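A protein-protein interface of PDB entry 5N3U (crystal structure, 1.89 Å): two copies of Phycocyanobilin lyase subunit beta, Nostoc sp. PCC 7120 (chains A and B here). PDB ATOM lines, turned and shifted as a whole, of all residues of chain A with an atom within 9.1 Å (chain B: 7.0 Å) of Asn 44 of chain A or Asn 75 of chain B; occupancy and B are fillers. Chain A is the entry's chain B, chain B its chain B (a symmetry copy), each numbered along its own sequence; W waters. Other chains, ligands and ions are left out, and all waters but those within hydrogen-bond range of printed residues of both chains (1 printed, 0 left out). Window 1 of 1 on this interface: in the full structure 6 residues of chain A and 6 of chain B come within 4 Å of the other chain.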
ATOM      1  N   ALA A  39      18.866 -11.195   7.857  1.00  0.00           N
ATOM      2  CA  ALA A  39      20.100 -10.784   8.503  1.00  0.00           C
ATOM      3  C   ALA A  39      20.137  -9.258   8.730  1.00  0.00           C
ATOM      4  O   ALA A  39      20.745  -8.819   9.659  1.00  0.00           O
ATOM      5  CB  ALA A  39      21.291 -11.211   7.685  1.00  0.00           C
ATOM      6  N   VAL A  40      19.445  -8.477   7.908  1.00  0.00           N
ATOM      7  CA  VAL A  40      19.385  -7.046   8.077  1.00  0.00           C
ATOM      8  C   VAL A  40      18.827  -6.679   9.464  1.00  0.00           C
ATOM      9  O   VAL A  40      19.195  -5.651   9.996  1.00  0.00           O
ATOM     10  CB  VAL A  40      18.585  -6.349   6.972  1.00  0.00           C
ATOM     11  CG1 VAL A  40      18.298  -4.896   7.301  1.00  0.00           C
ATOM     12  CG2 VAL A  40      19.365  -6.463   5.660  1.00  0.00           C
ATOM     13  N   PHE A  41      17.921  -7.478  10.022  1.00  0.00           N
ATOM     14  CA  PHE A  41      17.324  -7.117  11.326  1.00  0.00           C
ATOM     15  C   PHE A  41      18.382  -7.018  12.435  1.00  0.00           C
ATOM     16  O   PHE A  41      18.207  -6.337  13.412  1.00  0.00           O
ATOM     17  CB  PHE A  41      16.320  -8.163  11.753  1.00  0.00           C
ATOM     18  CG  PHE A  41      15.174  -8.423  10.834  1.00  0.00           C
ATOM     19  CD1 PHE A  41      14.669  -7.454   9.936  1.00  0.00           C
ATOM     20  CD2 PHE A  41      14.533  -9.634  10.921  1.00  0.00           C
ATOM     21  CE1 PHE A  41      13.548  -7.725   9.179  1.00  0.00           C
ATOM     22  CE2 PHE A  41      13.426  -9.923  10.147  1.00  0.00           C
ATOM     23  CZ  PHE A  41      12.924  -8.975   9.258  1.00  0.00           C
ATOM     24  N   GLY A  42      19.508  -7.649  12.271  1.00  0.00           N
ATOM     25  CA  GLY A  42      20.616  -7.606  13.198  1.00  0.00           C
ATOM     26  C   GLY A  42      21.446  -6.322  13.215  1.00  0.00           C
ATOM     27  O   GLY A  42      22.299  -6.189  14.060  1.00  0.00           O
ATOM     28  N   TYR A  43      21.195  -5.411  12.295  1.00  0.00           N
ATOM     29  CA  TYR A  43      21.884  -4.140  12.233  1.00  0.00           C
ATOM     30  C   TYR A  43      20.852  -3.148  12.638  1.00  0.00           C
ATOM     31  O   TYR A  43      19.808  -2.928  11.914  1.00  0.00           O
ATOM     32  CB  TYR A  43      22.229  -3.785  10.808  1.00  0.00           C
ATOM     33  CG  TYR A  43      22.994  -4.883  10.170  1.00  0.00           C
ATOM     34  CD1 TYR A  43      24.194  -5.398  10.729  1.00  0.00           C
ATOM     35  CD2 TYR A  43      22.524  -5.443   8.987  1.00  0.00           C
ATOM     36  CE1 TYR A  43      24.869  -6.449  10.087  1.00  0.00           C
ATOM     37  CE2 TYR A  43      23.193  -6.472   8.349  1.00  0.00           C
ATOM     38  CZ  TYR A  43      24.334  -6.974   8.885  1.00  0.00           C
ATOM     39  OH  TYR A  43      24.886  -8.003   8.162  1.00  0.00           O
ATOM     40  N   ASN A  44      21.122  -2.505  13.733  1.00  0.00           N
ATOM     41  CA  ASN A  44      20.026  -1.867  14.463  1.00  0.00           C
ATOM     42  C   ASN A  44      19.724  -0.538  13.896  1.00  0.00           C
ATOM     43  O   ASN A  44      19.989   0.522  14.491  1.00  0.00           O
ATOM     44  CB  ASN A  44      20.369  -1.684  15.940  1.00  0.00           C
ATOM     45  CG  ASN A  44      19.280  -0.918  16.671  1.00  0.00           C
ATOM     46  OD1 ASN A  44      18.088  -1.039  16.329  1.00  0.00           O
ATOM     47  ND2 ASN A  44      19.670  -0.093  17.632  1.00  0.00           N
ATOM     48  N   ASN A  45      19.209  -0.582  12.687  1.00  0.00           N
ATOM     49  CA  ASN A  45      18.809   0.559  12.004  1.00  0.00           C
ATOM     50  C   ASN A  45      17.344   0.318  11.665  1.00  0.00           C
ATOM     51  O   ASN A  45      17.045  -0.436  10.758  1.00  0.00           O
ATOM     52  CB  ASN A  45      19.622   0.732  10.726  1.00  0.00           C
ATOM     53  CG  ASN A  45      19.360   2.051  10.089  1.00  0.00           C
ATOM     54  OD1 ASN A  45      18.536   2.193   9.216  1.00  0.00           O
ATOM     55  ND2 ASN A  45      20.010   3.065  10.608  1.00  0.00           N
ATOM     56  N   PRO A  46      16.427   0.990  12.371  1.00  0.00           N
ATOM     57  CA  PRO A  46      15.037   0.739  12.149  1.00  0.00           C
ATOM     58  C   PRO A  46      14.536   1.036  10.788  1.00  0.00           C
ATOM     59  O   PRO A  46      13.639   0.336  10.313  1.00  0.00           O
ATOM     60  CB  PRO A  46      14.358   1.662  13.123  1.00  0.00           C
ATOM     61  CG  PRO A  46      15.315   1.682  14.240  1.00  0.00           C
ATOM     62  CD  PRO A  46      16.632   1.790  13.587  1.00  0.00           C
ATOM     63  N   THR A  47      15.071   2.068  10.168  1.00  0.00           N
ATOM     64  CA  THR A  47      14.735   2.340   8.792  1.00  0.00           C
ATOM     65  C   THR A  47      15.074   1.159   7.846  1.00  0.00           C
ATOM     66  O   THR A  47      14.199   0.685   7.155  1.00  0.00           O
ATOM     67  CB  THR A  47      15.428   3.650   8.320  1.00  0.00           C
ATOM     68  OG1 THR A  47      15.135   4.671   9.280  1.00  0.00           O
ATOM     69  CG2 THR A  47      14.875   4.104   6.959  1.00  0.00           C
ATOM     70  N   ALA A  48      16.322   0.698   7.845  1.00  0.00           N
ATOM     71  CA  ALA A  48      16.763  -0.427   7.044  1.00  0.00           C
ATOM     72  C   ALA A  48      15.975  -1.720   7.412  1.00  0.00           C
ATOM     73  O   ALA A  48      15.547  -2.480   6.542  1.00  0.00           O
ATOM     74  CB  ALA A  48      18.260  -0.704   7.246  1.00  0.00           C
ATOM     75  N   ALA A  49      15.850  -2.007   8.693  1.00  0.00           N
ATOM     76  CA  ALA A  49      15.102  -3.195   9.115  1.00  0.00           C
ATOM     77  C   ALA A  49      13.677  -3.109   8.608  1.00  0.00           C
ATOM     78  O   ALA A  49      13.129  -4.089   8.074  1.00  0.00           O
ATOM     79  CB  ALA A  49      15.153  -3.333  10.638  1.00  0.00           C
ATOM     80  N   ALA A  50      13.040  -1.962   8.749  1.00  0.00           N
ATOM     81  CA  ALA A  50      11.625  -1.847   8.321  1.00  0.00           C
ATOM     82  C   ALA A  50      11.466  -2.064   6.814  1.00  0.00           C
ATOM     83  O   ALA A  50      10.512  -2.692   6.362  1.00  0.00           O
ATOM     84  CB  ALA A  50      11.017  -0.526   8.753  1.00  0.00           C
ATOM     85  N   ASN A  75      19.648 -11.518  19.936  1.00  0.00           N
ATOM     86  CA  ASN A  75      19.492 -10.105  19.705  1.00  0.00           C
ATOM     87  C   ASN A  75      18.013  -9.822  19.702  1.00  0.00           C
ATOM     88  O   ASN A  75      17.361 -10.059  18.673  1.00  0.00           O
ATOM     89  CB  ASN A  75      20.248  -9.638  18.411  1.00  0.00           C
ATOM     90  CG  ASN A  75      19.998  -8.188  18.063  1.00  0.00           C
ATOM     91  OD1 ASN A  75      19.099  -7.553  18.536  1.00  0.00           O
ATOM     92  ND2 ASN A  75      20.784  -7.669  17.164  1.00  0.00           N
ATOM     93  N   TYR A  76      17.487  -9.278  20.804  1.00  0.00           N
ATOM     94  CA  TYR A  76      16.077  -9.058  20.923  1.00  0.00           C
ATOM     95  C   TYR A  76      15.586  -8.033  19.882  1.00  0.00           C
ATOM     96  O   TYR A  76      14.436  -8.116  19.468  1.00  0.00           O
ATOM     97  CB  TYR A  76      15.628  -8.672  22.329  1.00  0.00           C
ATOM     98  CG  TYR A  76      16.060  -7.330  22.826  1.00  0.00           C
ATOM     99  CD1 TYR A  76      15.403  -6.191  22.436  1.00  0.00           C
ATOM    100  CD2 TYR A  76      17.183  -7.200  23.683  1.00  0.00           C
ATOM    101  CE1 TYR A  76      15.822  -4.914  22.857  1.00  0.00           C
ATOM    102  CE2 TYR A  76      17.592  -5.940  24.115  1.00  0.00           C
ATOM    103  CZ  TYR A  76      16.942  -4.812  23.655  1.00  0.00           C
ATOM    104  OH  TYR A  76      17.331  -3.607  24.112  1.00  0.00           O
ATOM    105  N   GLY A  77      16.441  -7.101  19.511  1.00  0.00           N
ATOM    106  CA  GLY A  77      16.043  -6.034  18.531  1.00  0.00           C
ATOM    107  C   GLY A  77      15.706  -6.707  17.228  1.00  0.00           C
ATOM    108  O   GLY A  77      14.629  -6.462  16.622  1.00  0.00           O
ATOM    109  N   ALA A  78      16.585  -7.609  16.836  1.00  0.00           N
ATOM    110  CA  ALA A  78      16.367  -8.359  15.558  1.00  0.00           C
ATOM    111  C   ALA A  78      15.205  -9.288  15.624  1.00  0.00           C
ATOM    112  O   ALA A  78      14.392  -9.390  14.706  1.00  0.00           O
ATOM    113  CB  ALA A  78      17.603  -9.137  15.252  1.00  0.00           C
ATOM    114  N   TYR A  81      11.732  -7.951  14.995  1.00  0.00           N
ATOM    115  CA  TYR A  81      11.446  -7.794  13.568  1.00  0.00           C
ATOM    116  C   TYR A  81      11.057  -9.097  12.955  1.00  0.00           C
ATOM    117  O   TYR A  81      10.115  -9.124  12.147  1.00  0.00           O
ATOM    118  CB  TYR A  81      12.641  -7.202  12.783  1.00  0.00           C
ATOM    119  CG  TYR A  81      12.788  -5.730  13.011  1.00  0.00           C
ATOM    120  CD1 TYR A  81      11.857  -4.837  12.464  1.00  0.00           C
ATOM    121  CD2 TYR A  81      13.865  -5.207  13.735  1.00  0.00           C
ATOM    122  CE1 TYR A  81      11.984  -3.455  12.660  1.00  0.00           C
ATOM    123  CE2 TYR A  81      14.020  -3.820  13.944  1.00  0.00           C
ATOM    124  CZ  TYR A  81      13.048  -2.959  13.417  1.00  0.00           C
ATOM    125  OH  TYR A  81      13.197  -1.582  13.571  1.00  0.00           O
ATOM    126  N   PHE B  41      27.817   3.261  18.342  1.00  0.00           N
ATOM    127  CA  PHE B  41      27.696   1.982  19.076  1.00  0.00           C
ATOM    128  C   PHE B  41      26.271   1.414  19.011  1.00  0.00           C
ATOM    129  O   PHE B  41      26.058   0.237  19.137  1.00  0.00           O
ATOM    130  CB  PHE B  41      28.036   2.180  20.537  1.00  0.00           C
ATOM    131  CG  PHE B  41      29.394   2.709  20.855  1.00  0.00           C
ATOM    132  CD1 PHE B  41      30.512   2.525  20.010  1.00  0.00           C
ATOM    133  CD2 PHE B  41      29.579   3.338  22.061  1.00  0.00           C
ATOM    134  CE1 PHE B  41      31.761   2.959  20.405  1.00  0.00           C
ATOM    135  CE2 PHE B  41      30.820   3.800  22.453  1.00  0.00           C
ATOM    136  CZ  PHE B  41      31.927   3.625  21.625  1.00  0.00           C
ATOM    137  N   GLY B  42      25.292   2.233  18.758  1.00  0.00           N
ATOM    138  CA  GLY B  42      23.910   1.839  18.611  1.00  0.00           C
ATOM    139  C   GLY B  42      23.533   1.134  17.307  1.00  0.00           C
ATOM    140  O   GLY B  42      22.422   0.672  17.193  1.00  0.00           O
ATOM    141  N   TYR B  43      24.443   1.066  16.355  1.00  0.00           N
ATOM    142  CA  TYR B  43      24.219   0.390  15.096  1.00  0.00           C
ATOM    143  C   TYR B  43      25.081  -0.820  15.176  1.00  0.00           C
ATOM    144  O   TYR B  43      26.366  -0.732  15.213  1.00  0.00           O
ATOM    145  CB  TYR B  43      24.780   1.193  13.948  1.00  0.00           C
ATOM    146  CG  TYR B  43      24.235   2.571  13.963  1.00  0.00           C
ATOM    147  CD1 TYR B  43      22.840   2.836  13.959  1.00  0.00           C
ATOM    148  CD2 TYR B  43      25.111   3.651  13.993  1.00  0.00           C
ATOM    149  CE1 TYR B  43      22.380   4.163  13.988  1.00  0.00           C
ATOM    150  CE2 TYR B  43      24.660   4.958  14.012  1.00  0.00           C
ATOM    151  CZ  TYR B  43      23.328   5.216  14.019  1.00  0.00           C
ATOM    152  OH  TYR B  43      23.017   6.553  14.057  1.00  0.00           O
ATOM    153  N   ASN B  44      24.433  -1.946  15.152  1.00  0.00           N
ATOM    154  CA  ASN B  44      25.090  -3.146  15.671  1.00  0.00           C
ATOM    155  C   ASN B  44      25.953  -3.756  14.641  1.00  0.00           C
ATOM    156  O   ASN B  44      25.675  -4.832  14.083  1.00  0.00           O
ATOM    157  CB  ASN B  44      24.069  -4.194  16.114  1.00  0.00           C
ATOM    158  CG  ASN B  44      24.750  -5.482  16.543  1.00  0.00           C
ATOM    159  OD1 ASN B  44      25.872  -5.451  17.084  1.00  0.00           O
ATOM    160  ND2 ASN B  44      24.120  -6.614  16.264  1.00  0.00           N
ATOM    161  N   ASN B  45      27.003  -3.028  14.331  1.00  0.00           N
ATOM    162  CA  ASN B  45      27.965  -3.453  13.423  1.00  0.00           C
ATOM    163  C   ASN B  45      29.278  -3.406  14.192  1.00  0.00           C
ATOM    164  O   ASN B  45      29.822  -2.338  14.402  1.00  0.00           O
ATOM    165  CB  ASN B  45      28.023  -2.511  12.226  1.00  0.00           C
ATOM    166  CG  ASN B  45      28.890  -3.057  11.146  1.00  0.00           C
ATOM    167  OD1 ASN B  45      30.057  -2.761  11.044  1.00  0.00           O
ATOM    168  ND2 ASN B  45      28.328  -3.959  10.376  1.00  0.00           N
ATOM    169  N   ILE B  71      25.546   7.211  27.905  1.00  0.00           N
ATOM    170  CA  ILE B  71      25.513   5.768  27.931  1.00  0.00           C
ATOM    171  C   ILE B  71      24.099   5.350  27.505  1.00  0.00           C
ATOM    172  O   ILE B  71      23.103   5.878  28.005  1.00  0.00           O
ATOM    173  CB  ILE B  71      25.860   5.213  29.282  1.00  0.00           C
ATOM    174  CG1 ILE B  71      27.328   5.478  29.521  1.00  0.00           C
ATOM    175  CG2 ILE B  71      25.614   3.704  29.300  1.00  0.00           C
ATOM    176  CD1 ILE B  71      27.746   5.189  30.912  1.00  0.00           C
ATOM    177  N   ASP B  72      24.029   4.399  26.569  1.00  0.00           N
ATOM    178  CA  ASP B  72      22.733   3.912  26.089  1.00  0.00           C
ATOM    179  C   ASP B  72      22.224   2.836  27.102  1.00  0.00           C
ATOM    180  O   ASP B  72      22.604   1.659  27.035  1.00  0.00           O
ATOM    181  CB  ASP B  72      22.835   3.334  24.698  1.00  0.00           C
ATOM    182  CG  ASP B  72      21.473   3.124  24.028  1.00  0.00           C
ATOM    183  OD1 ASP B  72      20.447   2.972  24.734  1.00  0.00           O
ATOM    184  OD2 ASP B  72      21.454   3.053  22.776  1.00  0.00           O
ATOM    185  N   ASP B  73      21.328   3.277  27.949  1.00  0.00           N
ATOM    186  CA  ASP B  73      20.673   2.371  28.949  1.00  0.00           C
ATOM    187  C   ASP B  73      19.618   1.493  28.380  1.00  0.00           C
ATOM    188  O   ASP B  73      19.052   0.739  29.110  1.00  0.00           O
ATOM    189  CB  ASP B  73      20.120   3.176  30.126  1.00  0.00           C
ATOM    190  CG  ASP B  73      21.260   3.702  31.010  1.00  0.00           C
ATOM    191  OD1 ASP B  73      22.282   2.995  31.074  1.00  0.00           O
ATOM    192  OD2 ASP B  73      21.160   4.807  31.523  1.00  0.00           O
ATOM    193  N   TYR B  74      19.391   1.563  27.072  1.00  0.00           N
ATOM    194  CA  TYR B  74      18.378   0.736  26.450  1.00  0.00           C
ATOM    195  C   TYR B  74      18.860  -0.137  25.342  1.00  0.00           C
ATOM    196  O   TYR B  74      18.016  -0.703  24.594  1.00  0.00           O
ATOM    197  CB  TYR B  74      17.283   1.673  25.953  1.00  0.00           C
ATOM    198  CG  TYR B  74      16.828   2.562  27.100  1.00  0.00           C
ATOM    199  CD1 TYR B  74      15.849   2.133  27.991  1.00  0.00           C
ATOM    200  CD2 TYR B  74      17.345   3.827  27.277  1.00  0.00           C
ATOM    201  CE1 TYR B  74      15.440   2.925  29.057  1.00  0.00           C
ATOM    202  CE2 TYR B  74      16.935   4.620  28.330  1.00  0.00           C
ATOM    203  CZ  TYR B  74      15.980   4.151  29.194  1.00  0.00           C
ATOM    204  OH  TYR B  74      15.578   4.947  30.187  1.00  0.00           O
ATOM    205  N   ASN B  75      20.183  -0.248  25.198  1.00  0.00           N
ATOM    206  CA  ASN B  75      20.770  -1.110  24.206  1.00  0.00           C
ATOM    207  C   ASN B  75      22.042  -1.658  24.796  1.00  0.00           C
ATOM    208  O   ASN B  75      23.062  -0.952  24.781  1.00  0.00           O
ATOM    209  CB  ASN B  75      20.955  -0.376  22.830  1.00  0.00           C
ATOM    210  CG  ASN B  75      21.689  -1.207  21.802  1.00  0.00           C
ATOM    211  OD1 ASN B  75      22.321  -2.183  22.089  1.00  0.00           O
ATOM    212  ND2 ASN B  75      21.651  -0.769  20.576  1.00  0.00           N
ATOM    213  N   TYR B  76      22.015  -2.910  25.266  1.00  0.00           N
ATOM    214  CA  TYR B  76      23.150  -3.481  25.926  1.00  0.00           C
ATOM    215  C   TYR B  76      24.347  -3.603  24.962  1.00  0.00           C
ATOM    216  O   TYR B  76      25.482  -3.540  25.419  1.00  0.00           O
ATOM    217  CB  TYR B  76      22.861  -4.810  26.615  1.00  0.00           C
ATOM    218  CG  TYR B  76      22.567  -5.976  25.728  1.00  0.00           C
ATOM    219  CD1 TYR B  76      23.581  -6.659  25.106  1.00  0.00           C
ATOM    220  CD2 TYR B  76      21.230  -6.380  25.478  1.00  0.00           C
ATOM    221  CE1 TYR B  76      23.322  -7.732  24.230  1.00  0.00           C
ATOM    222  CE2 TYR B  76      20.969  -7.450  24.625  1.00  0.00           C
ATOM    223  CZ  TYR B  76      22.012  -8.077  23.971  1.00  0.00           C
ATOM    224  OH  TYR B  76      21.741  -9.130  23.178  1.00  0.00           O
ATOM    225  N   GLY B  77      24.072  -3.795  23.688  1.00  0.00           N
ATOM    226  CA  GLY B  77      25.170  -3.965  22.678  1.00  0.00           C
ATOM    227  C   GLY B  77      25.976  -2.694  22.653  1.00  0.00           C
ATOM    228  O   GLY B  77      27.232  -2.710  22.751  1.00  0.00           O
ATOM    229  N   ALA B  78      25.254  -1.592  22.599  1.00  0.00           N
ATOM    230  CA  ALA B  78      25.930  -0.255  22.575  1.00  0.00           C
ATOM    231  C   ALA B  78      26.617   0.067  23.856  1.00  0.00           C
ATOM    232  O   ALA B  78      27.742   0.566  23.891  1.00  0.00           O
ATOM    233  CB  ALA B  78      24.902   0.788  22.292  1.00  0.00           C
ATOM    234  N   ARG B  79      25.957  -0.288  24.968  1.00  0.00           N
ATOM    235  CA  ARG B  79      26.455   0.011  26.284  1.00  0.00           C
ATOM    236  C   ARG B  79      27.781  -0.668  26.561  1.00  0.00           C
ATOM    237  O   ARG B  79      28.657  -0.087  27.224  1.00  0.00           O
ATOM    238  CB  ARG B  79      25.360  -0.338  27.313  1.00  0.00           C
ATOM    239  CG  ARG B  79      25.700   0.024  28.706  1.00  0.00           C
ATOM    240  CD  ARG B  79      24.438   0.101  29.608  1.00  0.00           C
ATOM    241  NE  ARG B  79      23.831  -1.202  29.867  1.00  0.00           N
ATOM    242  CZ  ARG B  79      22.720  -1.712  29.291  1.00  0.00           C
ATOM    243  NH1 ARG B  79      22.315  -2.911  29.652  1.00  0.00           N
ATOM    244  NH2 ARG B  79      22.038  -1.058  28.319  1.00  0.00           N
ATOM    245  N   ALA B  80      27.958  -1.879  26.044  1.00  0.00           N
ATOM    246  CA  ALA B  80      29.117  -2.625  26.257  1.00  0.00           C
ATOM    247  C   ALA B  80      30.312  -1.884  25.623  1.00  0.00           C
ATOM    248  O   ALA B  80      31.379  -1.907  26.151  1.00  0.00           O
ATOM    249  CB  ALA B  80      28.979  -3.976  25.609  1.00  0.00           C
ATOM    250  N   VAL B 110      28.413  -6.420  29.084  1.00  0.00           N
ATOM    251  CA  VAL B 110      28.643  -5.138  29.776  1.00  0.00           C
ATOM    252  C   VAL B 110      29.420  -5.357  31.049  1.00  0.00           C
ATOM    253  O   VAL B 110      30.371  -4.627  31.338  1.00  0.00           O
ATOM    254  CB  VAL B 110      27.328  -4.446  30.070  1.00  0.00           C
ATOM    255  CG1 VAL B 110      27.532  -3.261  31.043  1.00  0.00           C
ATOM    256  CG2 VAL B 110      26.706  -3.980  28.808  1.00  0.00           C
HETATM  257  O   HOH W   1      17.670  -1.703  21.918  1.00  0.00           O
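O of Gly 42 of chain A sits at hydrogen-bond distance from ND2 of Asn 44 of chain B (2.9 Å).
The side-chain amide nitrogen (ND2) of Asn 44 of chain A is in hydrogen-bond range of the backbone carbonyl oxygen (O) of Gly 42 of chain B (2.9 Å).
O of Tyr 74 of chain B is in hydrogen-bond range of OH of Tyr 76 of chain A, at 3.0 Å.
The side-chain amide oxygen (OD1) of Asn 75 of chain A sits at hydrogen-bond distance from the backbone NH (N) of Gly 77 of chain A (2.9 Å).
The backbone NH of Ala 78 of chain A lies within hydrogen-bond range of the side-chain amide oxygen of Asn 75 of chain A, 3.0 Å away.
OD1 of Asp 72 of chain B sits at hydrogen-bond distance from N of Tyr 74 of chain B (2.9 Å).
OD1 of Asp 72 of chain B sits at hydrogen-bond distance from N of Asn 75 of chain B (3.3 Å).
The side-chain amide oxygen (OD1) of Asn 75 of chain B sits at hydrogen-bond distance from the backbone NH (N) of Gly 77 of chain B (2.9 Å).
The side-chain amide oxygen (OD1) of Asn 75 of chain B sits at hydrogen-bond distance from the backbone NH (N) of Ala 78 of chain B (3.0 Å).
Tyr 43 of chain A touches Asn 44 of chain B (CD1 to O, 3.7 Å).
CD1 of Tyr 43 of chain B touches O of Asn 44 of chain A (3.7 Å).
Asn 44 of chain A touches Asn 44 of chain B.
Asn 44 of chain A touches Asn 75 of chain B (ND2 to ND2, 3.6 Å).
Asn 44 of chain B touches Asn 75 of chain A.
CE2 of Tyr 76 of chain B touches CE2 of Tyr 76 of chain A, 3.7 Å away.
Asn 44 of chain A touches just these residues of chain B: Gly 42 (2.9 Å), Tyr 43 (3.7 Å), Asn 44 (3.6 Å) and Asn 75 (3.6 Å).
Of the printed residues of chain B, Asn 75 of chain A touches Asn 44.
Of the printed residues of chain A, Gly 42 of chain B touches Asn 44 (2.9 Å).
Printed residues of chain A within 4 Å of Asn 44 of chain B: Gly 42 (2.9 Å), Tyr 43 (3.7 Å), Asn 44 (3.6 Å) and Asn 75 (3.6 Å).
Asn 45 of chain B touches none of the printed residues of chain A.
Of the printed residues of chain A, Tyr 74 of chain B touches Tyr 76.
Of chain A, only Asn 44 (3.6 Å) comes within 4 Å of Asn 75 of chain B.
Of the printed residues of chain A, Tyr 76 of chain B touches Tyr 76.
No residue of chain A comes within 4 Å of Gly 77 of chain B.
Ala 78 of chain B touches none of the printed residues of chain A.
The nearest residue of chain B that does not touch Asn 44 of chain A is Asn 45 of chain B (5.9 Å).
The nearest printed residue of chain B that does not touch Asn 75 of chain A is Tyr 76 of chain B (4.3 Å).
Of the 16 printed residues of chain B, 6 touch a printed residue of chain A.
Hydrophobic or aromatic side chains of chain B that line the printed part of chain A: Tyr 43 and Tyr 76.
Printed residues of chain A that touch a printed residue of chain B: Gly 42, Tyr 43, Asn 44, Asn 75 and Tyr 76.
Along chain A the printed residues that touch a printed residue of chain B span positions 42 to 76.
Tyr 43 of chain A touches Asn 44 of chain B, and with the chains exchanged Asn 44 of chain A touches Tyr 43 of chain B.
Asn 44 of chain A touches its own counterpart, Asn 44 of chain B.
Asn 44 of chain A touches Asn 75 of chain B, and with the chains exchanged Asn 75 of chain A touches Asn 44 of chain B.
Tyr 76 of chain A touches its own counterpart, Tyr 76 of chain B.
9 positions are printed for both chains.
Of the 9 pairs that touch across the chains among the printed residues, 8 have their exchanged pair printed and touching as well.
Water W1 lies within hydrogen-bond range of O of Tyr 74 of chain B (2.9 Å) and OH of Tyr 76 of chain A (2.9 Å).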
